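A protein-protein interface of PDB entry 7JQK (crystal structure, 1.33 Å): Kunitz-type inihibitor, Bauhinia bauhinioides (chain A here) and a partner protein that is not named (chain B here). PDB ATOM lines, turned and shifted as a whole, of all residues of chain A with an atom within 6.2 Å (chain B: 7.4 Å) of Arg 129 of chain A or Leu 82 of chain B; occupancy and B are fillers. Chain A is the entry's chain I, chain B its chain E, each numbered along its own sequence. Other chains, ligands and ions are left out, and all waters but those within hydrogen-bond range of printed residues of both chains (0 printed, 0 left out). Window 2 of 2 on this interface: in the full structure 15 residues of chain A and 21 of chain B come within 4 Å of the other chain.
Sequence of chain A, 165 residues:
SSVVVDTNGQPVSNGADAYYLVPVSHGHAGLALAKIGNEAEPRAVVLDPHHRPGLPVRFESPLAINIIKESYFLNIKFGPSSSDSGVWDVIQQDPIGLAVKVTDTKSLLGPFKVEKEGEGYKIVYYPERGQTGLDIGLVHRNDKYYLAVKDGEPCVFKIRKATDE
The backbone carbonyl oxygen (O) of Arg 80 of chain B sits at hydrogen-bond distance from the side-chain amide nitrogen (ND2) of Asn 85 of chain B (3.3 Å). The backbone carbonyl oxygen of Leu 109 of chain A sits at hydrogen-bond distance from the guanidinium group of Arg 129 of chain A, 2.8 Å away. O of Gly 110 of chain A lies within hydrogen-bond range of NE of Arg 129 of chain A.
Among the printed residues, merely in contact across the chains: Phe 73 of chain A with Leu 82 of chain B (3.97 Å), Leu 109 of chain A with Leu 82 of chain B (3.9 Å), Arg 129 of chain A with Leu 82 of chain B (3.8 Å) and Gln 131 of chain A with Arg 80 of chain B (3.99 Å).
Of the printed residues of chain B, Arg 129 of chain A touches Leu 82 (3.8 Å). Of the printed residues of chain A, Leu 82 of chain B touches Phe 73, Leu 109 and Arg 129. No residue of chain B comes within 4 Å of Gly 130 of chain A. Printed residues of chain B within 4 Å of Leu 109 of chain A: Leu 82. Printed residues of chain B within 4 Å of Phe 73 of chain A: Leu 82 (3.97 Å). Of the printed residues of chain A, Arg 80 of chain B touches Gln 131 (3.99 Å). Printed residues of chain B within 4 Å of Gln 131 of chain A: Arg 80 (3.99 Å). Pro 81 of chain B touches none of the printed residues of chain A. Pro 154 of chain B touches none of the printed residues of chain A. The nearest printed residue of chain B that does not touch Arg 129 of chain A is Leu 155 of chain B (7.6 Å). The nearest printed residue of chain A that does not touch Leu 82 of chain B is Glu 128 of chain A (5.5 Å). The nearest printed residue of chain B that does not touch Gln 131 of chain A is Leu 82 of chain B (8.0 Å).
Of the 15 printed residues of chain B, 2 touch a printed residue of chain A. Among the printed residues, 4 pairs touch across the chains. Among the printed residues, no Asp or Glu carboxylate lies within 4 Å of a Lys or Arg side-chain nitrogen of the other chain.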
ATOM      1  N   PHE A  73     -12.667   5.729 -12.488  1.00  0.00           N
ATOM      2  CA  PHE A  73     -12.475   7.191 -12.430  1.00  0.00           C
ATOM      3  C   PHE A  73     -13.590   7.848 -11.606  1.00  0.00           C
ATOM      4  O   PHE A  73     -14.788   7.545 -11.823  1.00  0.00           O
ATOM      5  CB  PHE A  73     -12.506   7.794 -13.827  1.00  0.00           C
ATOM      6  CG  PHE A  73     -11.151   7.745 -14.478  1.00  0.00           C
ATOM      7  CD1 PHE A  73     -10.085   8.414 -13.857  1.00  0.00           C
ATOM      8  CD2 PHE A  73     -10.950   7.078 -15.693  1.00  0.00           C
ATOM      9  CE1 PHE A  73      -8.842   8.393 -14.443  1.00  0.00           C
ATOM     10  CE2 PHE A  73      -9.692   7.097 -16.320  1.00  0.00           C
ATOM     11  CZ  PHE A  73      -8.650   7.792 -15.671  1.00  0.00           C
ATOM     12  N   ASN A  75     -15.211  11.426  -9.462  1.00  0.00           N
ATOM     13  CA  ASN A  75     -15.232  12.777  -8.865  1.00  0.00           C
ATOM     14  C   ASN A  75     -15.186  12.620  -7.348  1.00  0.00           C
ATOM     15  O   ASN A  75     -15.688  11.630  -6.779  1.00  0.00           O
ATOM     16  CB  ASN A  75     -16.542  13.498  -9.236  1.00  0.00           C
ATOM     17  CG  ASN A  75     -16.440  14.076 -10.627  1.00  0.00           C
ATOM     18  OD1 ASN A  75     -15.549  14.885 -10.876  1.00  0.00           O
ATOM     19  ND2 ASN A  75     -17.319  13.677 -11.558  1.00  0.00           N
ATOM     20  N   ASP A  89     -10.786  19.465  -8.188  1.00  0.00           N
ATOM     21  CA  ASP A  89     -10.021  19.407  -9.426  1.00  0.00           C
ATOM     22  C   ASP A  89      -8.562  19.682  -9.085  1.00  0.00           C
ATOM     23  O   ASP A  89      -8.255  19.976  -7.922  1.00  0.00           O
ATOM     24  CB  ASP A  89     -10.472  20.460 -10.459  1.00  0.00           C
ATOM     25  CG  ASP A  89     -10.018  20.111 -11.906  1.00  0.00           C
ATOM     26  OD1 ASP A  89      -9.375  18.969 -12.166  1.00  0.00           O
ATOM     27  OD2 ASP A  89     -10.441  20.827 -12.775  1.00  0.00           O
ATOM     28  N   SER A 107     -17.361  17.243 -14.405  1.00  0.00           N
ATOM     29  CA  SER A 107     -17.482  16.406 -15.574  1.00  0.00           C
ATOM     30  C   SER A 107     -18.222  15.118 -15.228  1.00  0.00           C
ATOM     31  O   SER A 107     -18.260  14.696 -14.089  1.00  0.00           O
ATOM     32  CB  SER A 107     -16.086  16.110 -16.216  1.00  0.00           C
ATOM     33  OG  SER A 107     -15.364  17.310 -16.618  1.00  0.00           O
ATOM     34  N   LEU A 109     -17.299  12.204 -15.803  1.00  0.00           N
ATOM     35  CA  LEU A 109     -16.290  11.267 -15.302  1.00  0.00           C
ATOM     36  C   LEU A 109     -15.135  12.093 -14.743  1.00  0.00           C
ATOM     37  O   LEU A 109     -14.505  12.916 -15.440  1.00  0.00           O
ATOM     38  CB  LEU A 109     -15.957  10.442 -16.556  1.00  0.00           C
ATOM     39  CG  LEU A 109     -15.178   9.187 -16.302  1.00  0.00           C
ATOM     40  CD1 LEU A 109     -15.932   8.189 -15.413  1.00  0.00           C
ATOM     41  CD2 LEU A 109     -14.746   8.571 -17.633  1.00  0.00           C
ATOM     42  N   GLY A 110     -14.896  11.936 -13.439  1.00  0.00           N
ATOM     43  CA  GLY A 110     -13.844  12.721 -12.787  1.00  0.00           C
ATOM     44  C   GLY A 110     -12.466  12.139 -13.083  1.00  0.00           C
ATOM     45  O   GLY A 110     -12.309  11.099 -13.727  1.00  0.00           O
ATOM     46  N   PRO A 111     -11.417  12.821 -12.572  1.00  0.00           N
ATOM     47  CA  PRO A 111     -10.051  12.456 -12.934  1.00  0.00           C
ATOM     48  C   PRO A 111      -9.271  11.739 -11.830  1.00  0.00           C
ATOM     49  O   PRO A 111      -8.069  11.499 -11.978  1.00  0.00           O
ATOM     50  CB  PRO A 111      -9.436  13.847 -13.149  1.00  0.00           C
ATOM     51  CG  PRO A 111     -10.059  14.702 -12.036  1.00  0.00           C
ATOM     52  CD  PRO A 111     -11.516  14.184 -12.002  1.00  0.00           C
ATOM     53  N   PHE A 112      -9.941  11.333 -10.743  1.00  0.00           N
ATOM     54  CA  PHE A 112      -9.242  10.734  -9.622  1.00  0.00           C
ATOM     55  C   PHE A 112      -9.482   9.220  -9.606  1.00  0.00           C
ATOM     56  O   PHE A 112     -10.558   8.727 -10.031  1.00  0.00           O
ATOM     57  CB  PHE A 112      -9.754  11.332  -8.302  1.00  0.00           C
ATOM     58  CG  PHE A 112      -9.471  12.801  -8.190  1.00  0.00           C
ATOM     59  CD1 PHE A 112      -8.177  13.253  -7.891  1.00  0.00           C
ATOM     60  CD2 PHE A 112     -10.473  13.736  -8.398  1.00  0.00           C
ATOM     61  CE1 PHE A 112      -7.921  14.620  -7.802  1.00  0.00           C
ATOM     62  CE2 PHE A 112     -10.234  15.107  -8.300  1.00  0.00           C
ATOM     63  CZ  PHE A 112      -8.938  15.545  -7.979  1.00  0.00           C
ATOM     64  N   TYR A 125      -4.320  11.388  -9.255  1.00  0.00           N
ATOM     65  CA  TYR A 125      -4.927  12.285 -10.228  1.00  0.00           C
ATOM     66  C   TYR A 125      -4.404  11.896 -11.599  1.00  0.00           C
ATOM     67  O   TYR A 125      -3.186  11.792 -11.800  1.00  0.00           O
ATOM     68  CB  TYR A 125      -4.500  13.730  -9.890  1.00  0.00           C
ATOM     69  CG  TYR A 125      -4.796  14.705 -10.993  1.00  0.00           C
ATOM     70  CD1 TYR A 125      -6.106  14.975 -11.377  1.00  0.00           C
ATOM     71  CD2 TYR A 125      -3.730  15.359 -11.623  1.00  0.00           C
ATOM     72  CE1 TYR A 125      -6.375  15.852 -12.417  1.00  0.00           C
ATOM     73  CE2 TYR A 125      -4.020  16.252 -12.672  1.00  0.00           C
ATOM     74  CZ  TYR A 125      -5.324  16.462 -13.082  1.00  0.00           C
ATOM     75  OH  TYR A 125      -5.579  17.371 -14.082  1.00  0.00           O
ATOM     76  N   TYR A 126      -5.296  11.684 -12.572  1.00  0.00           N
ATOM     77  CA  TYR A 126      -4.874  11.299 -13.926  1.00  0.00           C
ATOM     78  C   TYR A 126      -5.177  12.477 -14.853  1.00  0.00           C
ATOM     79  O   TYR A 126      -6.344  12.686 -15.254  1.00  0.00           O
ATOM     80  CB  TYR A 126      -5.702  10.081 -14.401  1.00  0.00           C
ATOM     81  CG  TYR A 126      -5.295   8.825 -13.664  1.00  0.00           C
ATOM     82  CD1 TYR A 126      -5.719   8.559 -12.343  1.00  0.00           C
ATOM     83  CD2 TYR A 126      -4.471   7.900 -14.288  1.00  0.00           C
ATOM     84  CE1 TYR A 126      -5.248   7.417 -11.715  1.00  0.00           C
ATOM     85  CE2 TYR A 126      -4.031   6.745 -13.673  1.00  0.00           C
ATOM     86  CZ  TYR A 126      -4.441   6.490 -12.368  1.00  0.00           C
ATOM     87  OH  TYR A 126      -3.994   5.347 -11.783  1.00  0.00           O
ATOM     88  N   PRO A 127      -4.148  13.300 -15.232  1.00  0.00           N
ATOM     89  CA  PRO A 127      -4.421  14.384 -16.150  1.00  0.00           C
ATOM     90  C   PRO A 127      -5.120  13.830 -17.412  1.00  0.00           C
ATOM     91  O   PRO A 127      -4.685  12.805 -17.969  1.00  0.00           O
ATOM     92  CB  PRO A 127      -3.036  14.940 -16.509  1.00  0.00           C
ATOM     93  CG  PRO A 127      -2.056  14.329 -15.562  1.00  0.00           C
ATOM     94  CD  PRO A 127      -2.740  13.200 -14.775  1.00  0.00           C
ATOM     95  N   GLU A 128      -6.195  14.493 -17.819  1.00  0.00           N
ATOM     96  CA  GLU A 128      -6.916  14.114 -19.047  1.00  0.00           C
ATOM     97  C   GLU A 128      -7.515  12.707 -18.993  1.00  0.00           C
ATOM     98  O   GLU A 128      -8.003  12.223 -20.025  1.00  0.00           O
ATOM     99  CB  GLU A 128      -6.081  14.158 -20.342  1.00  0.00           C
ATOM    100  CG  GLU A 128      -5.204  15.405 -20.346  1.00  0.00           C
ATOM    101  CD  GLU A 128      -5.151  16.125 -21.652  1.00  0.00           C
ATOM    102  OE1 GLU A 128      -6.160  16.138 -22.379  1.00  0.00           O
ATOM    103  OE2 GLU A 128      -4.138  16.760 -21.832  1.00  0.00           O
ATOM    104  N   ARG A 129      -7.587  12.094 -17.803  1.00  0.00           N
ATOM    105  CA  ARG A 129      -8.118  10.739 -17.618  1.00  0.00           C
ATOM    106  C   ARG A 129      -7.356   9.775 -18.531  1.00  0.00           C
ATOM    107  O   ARG A 129      -7.933   8.838 -19.088  1.00  0.00           O
ATOM    108  CB  ARG A 129      -9.641  10.646 -17.832  1.00  0.00           C
ATOM    109  CG  ARG A 129     -10.433  11.315 -16.714  1.00  0.00           C
ATOM    110  CD  ARG A 129     -10.264  12.810 -16.814  1.00  0.00           C
ATOM    111  NE  ARG A 129     -11.428  13.407 -16.167  1.00  0.00           N
ATOM    112  CZ  ARG A 129     -11.539  14.669 -15.874  1.00  0.00           C
ATOM    113  NH1 ARG A 129     -12.674  15.055 -15.342  1.00  0.00           N
ATOM    114  NH2 ARG A 129     -10.543  15.526 -16.180  1.00  0.00           N
ATOM    115  N   GLY A 130      -6.065  10.047 -18.673  1.00  0.00           N
ATOM    116  CA  GLY A 130      -5.168   9.160 -19.393  1.00  0.00           C
ATOM    117  C   GLY A 130      -4.667   8.007 -18.494  1.00  0.00           C
ATOM    118  O   GLY A 130      -5.291   7.621 -17.459  1.00  0.00           O
ATOM    119  N   GLN A 131      -3.542   7.408 -18.903  1.00  0.00           N
ATOM    120  CA  GLN A 131      -3.040   6.211 -18.297  1.00  0.00           C
ATOM    121  C   GLN A 131      -2.098   6.551 -17.156  1.00  0.00           C
ATOM    122  O   GLN A 131      -1.908   5.692 -16.284  1.00  0.00           O
ATOM    123  CB  GLN A 131      -2.254   5.386 -19.315  1.00  0.00           C
ATOM    124  CG  GLN A 131      -2.597   3.946 -19.163  1.00  0.00           C
ATOM    125  CD  GLN A 131      -1.995   3.062 -20.213  1.00  0.00           C
ATOM    126  OE1 GLN A 131      -2.522   2.894 -21.350  1.00  0.00           O
ATOM    127  NE2 GLN A 131      -0.844   2.554 -19.852  1.00  0.00           N
ATOM    128  N   GLU B  77     -12.244  -4.968 -25.557  1.00  0.00           N
ATOM    129  CA  GLU B  77     -12.164  -3.530 -25.736  1.00  0.00           C
ATOM    130  C   GLU B  77     -12.862  -2.765 -24.628  1.00  0.00           C
ATOM    131  O   GLU B  77     -13.037  -1.557 -24.755  1.00  0.00           O
ATOM    132  CB  GLU B  77     -12.667  -3.090 -27.126  1.00  0.00           C
ATOM    133  CG  GLU B  77     -11.843  -3.656 -28.287  1.00  0.00           C
ATOM    134  CD  GLU B  77     -12.412  -3.011 -29.583  1.00  0.00           C
ATOM    135  OE1 GLU B  77     -13.115  -3.722 -30.356  1.00  0.00           O
ATOM    136  OE2 GLU B  77     -12.156  -1.735 -29.842  1.00  0.00           O
ATOM    137  N   TYR B  78     -13.222  -3.451 -23.519  1.00  0.00           N
ATOM    138  CA  TYR B  78     -13.855  -2.701 -22.435  1.00  0.00           C
ATOM    139  C   TYR B  78     -13.032  -1.475 -22.014  1.00  0.00           C
ATOM    140  O   TYR B  78     -11.792  -1.592 -21.730  1.00  0.00           O
ATOM    141  CB  TYR B  78     -14.051  -3.677 -21.264  1.00  0.00           C
ATOM    142  CG  TYR B  78     -14.466  -2.941 -20.022  1.00  0.00           C
ATOM    143  CD1 TYR B  78     -15.583  -2.057 -20.025  1.00  0.00           C
ATOM    144  CD2 TYR B  78     -13.748  -3.142 -18.841  1.00  0.00           C
ATOM    145  CE1 TYR B  78     -15.946  -1.355 -18.873  1.00  0.00           C
ATOM    146  CE2 TYR B  78     -14.095  -2.448 -17.695  1.00  0.00           C
ATOM    147  CZ  TYR B  78     -15.147  -1.536 -17.713  1.00  0.00           C
ATOM    148  OH  TYR B  78     -15.482  -0.909 -16.561  1.00  0.00           O
ATOM    149  N   ASN B  79     -13.713  -0.331 -21.903  1.00  0.00           N
ATOM    150  CA  ASN B  79     -13.140   0.895 -21.379  1.00  0.00           C
ATOM    151  C   ASN B  79     -12.153   1.545 -22.336  1.00  0.00           C
ATOM    152  O   ASN B  79     -11.509   2.502 -21.862  1.00  0.00           O
ATOM    153  CB  ASN B  79     -12.521   0.674 -19.992  1.00  0.00           C
ATOM    154  CG  ASN B  79     -13.185   1.417 -18.899  1.00  0.00           C
ATOM    155  OD1 ASN B  79     -14.066   2.236 -19.080  1.00  0.00           O
ATOM    156  ND2 ASN B  79     -12.774   1.105 -17.697  1.00  0.00           N
ATOM    157  N   ARG B  80     -12.150   1.141 -23.647  1.00  0.00           N
ATOM    158  CA  ARG B  80     -11.406   1.945 -24.599  1.00  0.00           C
ATOM    159  C   ARG B  80     -12.359   2.100 -25.792  1.00  0.00           C
ATOM    160  O   ARG B  80     -12.589   1.167 -26.564  1.00  0.00           O
ATOM    161  CB  ARG B  80     -10.088   1.249 -24.994  1.00  0.00           C
ATOM    162  CG  ARG B  80      -9.331   2.058 -26.043  1.00  0.00           C
ATOM    163  CD  ARG B  80      -7.970   1.208 -26.243  1.00  0.00           C
ATOM    164  NE  ARG B  80      -7.068   0.798 -25.108  1.00  0.00           N
ATOM    165  CZ  ARG B  80      -6.598   1.685 -24.193  1.00  0.00           C
ATOM    166  NH1 ARG B  80      -6.971   2.923 -24.309  1.00  0.00           N
ATOM    167  NH2 ARG B  80      -5.762   1.439 -23.160  1.00  0.00           N
ATOM    168  N   PRO B  81     -13.001   3.280 -26.011  1.00  0.00           N
ATOM    169  CA  PRO B  81     -12.779   4.485 -25.187  1.00  0.00           C
ATOM    170  C   PRO B  81     -13.444   4.359 -23.806  1.00  0.00           C
ATOM    171  O   PRO B  81     -14.166   3.372 -23.531  1.00  0.00           O
ATOM    172  CB  PRO B  81     -13.484   5.601 -25.991  1.00  0.00           C
ATOM    173  CG  PRO B  81     -14.540   4.847 -26.820  1.00  0.00           C
ATOM    174  CD  PRO B  81     -13.925   3.504 -27.138  1.00  0.00           C
ATOM    175  N   LEU B  82     -13.241   5.359 -22.921  1.00  0.00           N
ATOM    176  CA  LEU B  82     -13.674   5.208 -21.542  1.00  0.00           C
ATOM    177  C   LEU B  82     -15.187   4.965 -21.501  1.00  0.00           C
ATOM    178  O   LEU B  82     -15.962   5.631 -22.194  1.00  0.00           O
ATOM    179  CB  LEU B  82     -13.337   6.460 -20.734  1.00  0.00           C
ATOM    180  CG  LEU B  82     -11.832   6.676 -20.486  1.00  0.00           C
ATOM    181  CD1 LEU B  82     -11.549   8.036 -19.868  1.00  0.00           C
ATOM    182  CD2 LEU B  82     -11.259   5.539 -19.617  1.00  0.00           C
ATOM    183  N   LEU B  83     -15.594   3.985 -20.656  1.00  0.00           N
ATOM    184  CA  LEU B  83     -16.975   3.566 -20.426  1.00  0.00           C
ATOM    185  C   LEU B  83     -17.525   2.663 -21.522  1.00  0.00           C
ATOM    186  O   LEU B  83     -18.615   2.083 -21.318  1.00  0.00           O
ATOM    187  CB  LEU B  83     -17.970   4.731 -20.179  1.00  0.00           C
ATOM    188  CG  LEU B  83     -17.541   5.697 -19.064  1.00  0.00           C
ATOM    189  CD1 LEU B  83     -18.550   6.814 -18.966  1.00  0.00           C
ATOM    190  CD2 LEU B  83     -17.404   4.974 -17.738  1.00  0.00           C
ATOM    191  N   ALA B  84     -16.848   2.522 -22.680  1.00  0.00           N
ATOM    192  CA  ALA B  84     -17.417   1.797 -23.814  1.00  0.00           C
ATOM    193  C   ALA B  84     -17.203   0.282 -23.682  1.00  0.00           C
ATOM    194  O   ALA B  84     -16.402  -0.223 -22.854  1.00  0.00           O
ATOM    195  CB  ALA B  84     -16.727   2.286 -25.088  1.00  0.00           C
ATOM    196  N   ASN B  85     -17.942  -0.464 -24.530  1.00  0.00           N
ATOM    197  CA  ASN B  85     -17.797  -1.909 -24.638  1.00  0.00           C
ATOM    198  C   ASN B  85     -17.998  -2.574 -23.254  1.00  0.00           C
ATOM    199  O   ASN B  85     -17.215  -3.460 -22.830  1.00  0.00           O
ATOM    200  CB  ASN B  85     -16.431  -2.302 -25.240  1.00  0.00           C
ATOM    201  CG  ASN B  85     -16.240  -1.604 -26.579  1.00  0.00           C
ATOM    202  OD1 ASN B  85     -17.129  -1.704 -27.437  1.00  0.00           O
ATOM    203  ND2 ASN B  85     -15.148  -0.854 -26.703  1.00  0.00           N
ATOM    204  N   PRO B 154     -18.006  13.876 -25.191  1.00  0.00           N
ATOM    205  CA  PRO B 154     -17.178  12.956 -25.958  1.00  0.00           C
ATOM    206  C   PRO B 154     -17.107  11.484 -25.580  1.00  0.00           C
ATOM    207  O   PRO B 154     -16.172  10.799 -26.004  1.00  0.00           O
ATOM    208  CB  PRO B 154     -15.778  13.708 -25.602  1.00  0.00           C
ATOM    209  CG  PRO B 154     -15.873  14.048 -24.113  1.00  0.00           C
ATOM    210  CD  PRO B 154     -17.240  14.652 -24.173  1.00  0.00           C
ATOM    211  N   LEU B 155     -18.033  11.049 -24.725  1.00  0.00           N
ATOM    212  CA  LEU B 155     -18.004   9.683 -24.200  1.00  0.00           C
ATOM    213  C   LEU B 155     -19.046   8.800 -24.908  1.00  0.00           C
ATOM    214  O   LEU B 155     -19.127   7.609 -24.574  1.00  0.00           O
ATOM    215  CB  LEU B 155     -18.206   9.711 -22.686  1.00  0.00           C
ATOM    216  CG  LEU B 155     -17.041  10.309 -21.922  1.00  0.00           C
ATOM    217  CD1 LEU B 155     -17.360  10.426 -20.420  1.00  0.00           C
ATOM    218  CD2 LEU B 155     -15.762   9.491 -22.204  1.00  0.00           C
ATOM    219  N   TYR B 156     -19.857   9.301 -25.844  1.00  0.00           N
ATOM    220  CA  TYR B 156     -20.785   8.440 -26.585  1.00  0.00           C
ATOM    221  C   TYR B 156     -19.985   7.610 -27.589  1.00  0.00           C
ATOM    222  O   TYR B 156     -19.159   8.116 -28.369  1.00  0.00           O
ATOM    223  CB  TYR B 156     -21.887   9.247 -27.282  1.00  0.00           C
ATOM    224  CG  TYR B 156     -22.637   8.359 -28.247  1.00  0.00           C
ATOM    225  CD1 TYR B 156     -23.491   7.338 -27.789  1.00  0.00           C
ATOM    226  CD2 TYR B 156     -22.388   8.449 -29.619  1.00  0.00           C
ATOM    227  CE1 TYR B 156     -24.054   6.455 -28.733  1.00  0.00           C
ATOM    228  CE2 TYR B 156     -22.950   7.600 -30.562  1.00  0.00           C
ATOM    229  CZ  TYR B 156     -23.759   6.582 -30.093  1.00  0.00           C
ATOM    230  OH  TYR B 156     -24.286   5.656 -30.956  1.00  0.00           O
ATOM    231  N   HIS B 157     -20.244   6.302 -27.595  1.00  0.00           N
ATOM    232  CA  HIS B 157     -19.617   5.384 -28.530  1.00  0.00           C
ATOM    233  C   HIS B 157     -20.715   4.403 -28.992  1.00  0.00           C
ATOM    234  O   HIS B 157     -21.641   4.121 -28.206  1.00  0.00           O
ATOM    235  CB  HIS B 157     -18.499   4.605 -27.801  1.00  0.00           C
ATOM    236  CG  HIS B 157     -17.781   3.614 -28.660  1.00  0.00           C
ATOM    237  ND1 HIS B 157     -18.049   2.248 -28.589  1.00  0.00           N
ATOM    238  CD2 HIS B 157     -16.790   3.797 -29.580  1.00  0.00           C
ATOM    239  CE1 HIS B 157     -17.257   1.625 -29.449  1.00  0.00           C
ATOM    240  NE2 HIS B 157     -16.479   2.568 -30.081  1.00  0.00           N
ATOM    241  N   MET B 160     -22.874   1.815 -27.101  1.00  0.00           N
ATOM    242  CA  MET B 160     -23.839   2.347 -26.131  1.00  0.00           C
ATOM    243  C   MET B 160     -25.109   2.735 -26.901  1.00  0.00           C
ATOM    244  O   MET B 160     -25.044   3.083 -28.099  1.00  0.00           O
ATOM    245  CB  MET B 160     -23.302   3.653 -25.516  1.00  0.00           C
ATOM    246  CG  MET B 160     -21.941   3.443 -24.819  1.00  0.00           C
ATOM    247  SD  MET B 160     -21.282   5.117 -24.476  1.00  0.00           S
ATOM    248  CE  MET B 160     -19.675   4.650 -23.766  1.00  0.00           C
ATOM    249  N   PHE B 193     -24.503   3.239 -17.431  1.00  0.00           N
ATOM    250  CA  PHE B 193     -24.102   4.447 -16.700  1.00  0.00           C
ATOM    251  C   PHE B 193     -25.073   5.578 -16.985  1.00  0.00           C
ATOM    252  O   PHE B 193     -25.931   5.444 -17.889  1.00  0.00           O
ATOM    253  CB  PHE B 193     -22.621   4.864 -16.976  1.00  0.00           C
ATOM    254  CG  PHE B 193     -22.376   5.415 -18.369  1.00  0.00           C
ATOM    255  CD1 PHE B 193     -22.067   4.555 -19.429  1.00  0.00           C
ATOM    256  CD2 PHE B 193     -22.473   6.787 -18.615  1.00  0.00           C
ATOM    257  CE1 PHE B 193     -21.782   5.040 -20.712  1.00  0.00           C
ATOM    258  CE2 PHE B 193     -22.217   7.302 -19.893  1.00  0.00           C
ATOM    259  CZ  PHE B 193     -21.867   6.420 -20.925  1.00  0.00           C
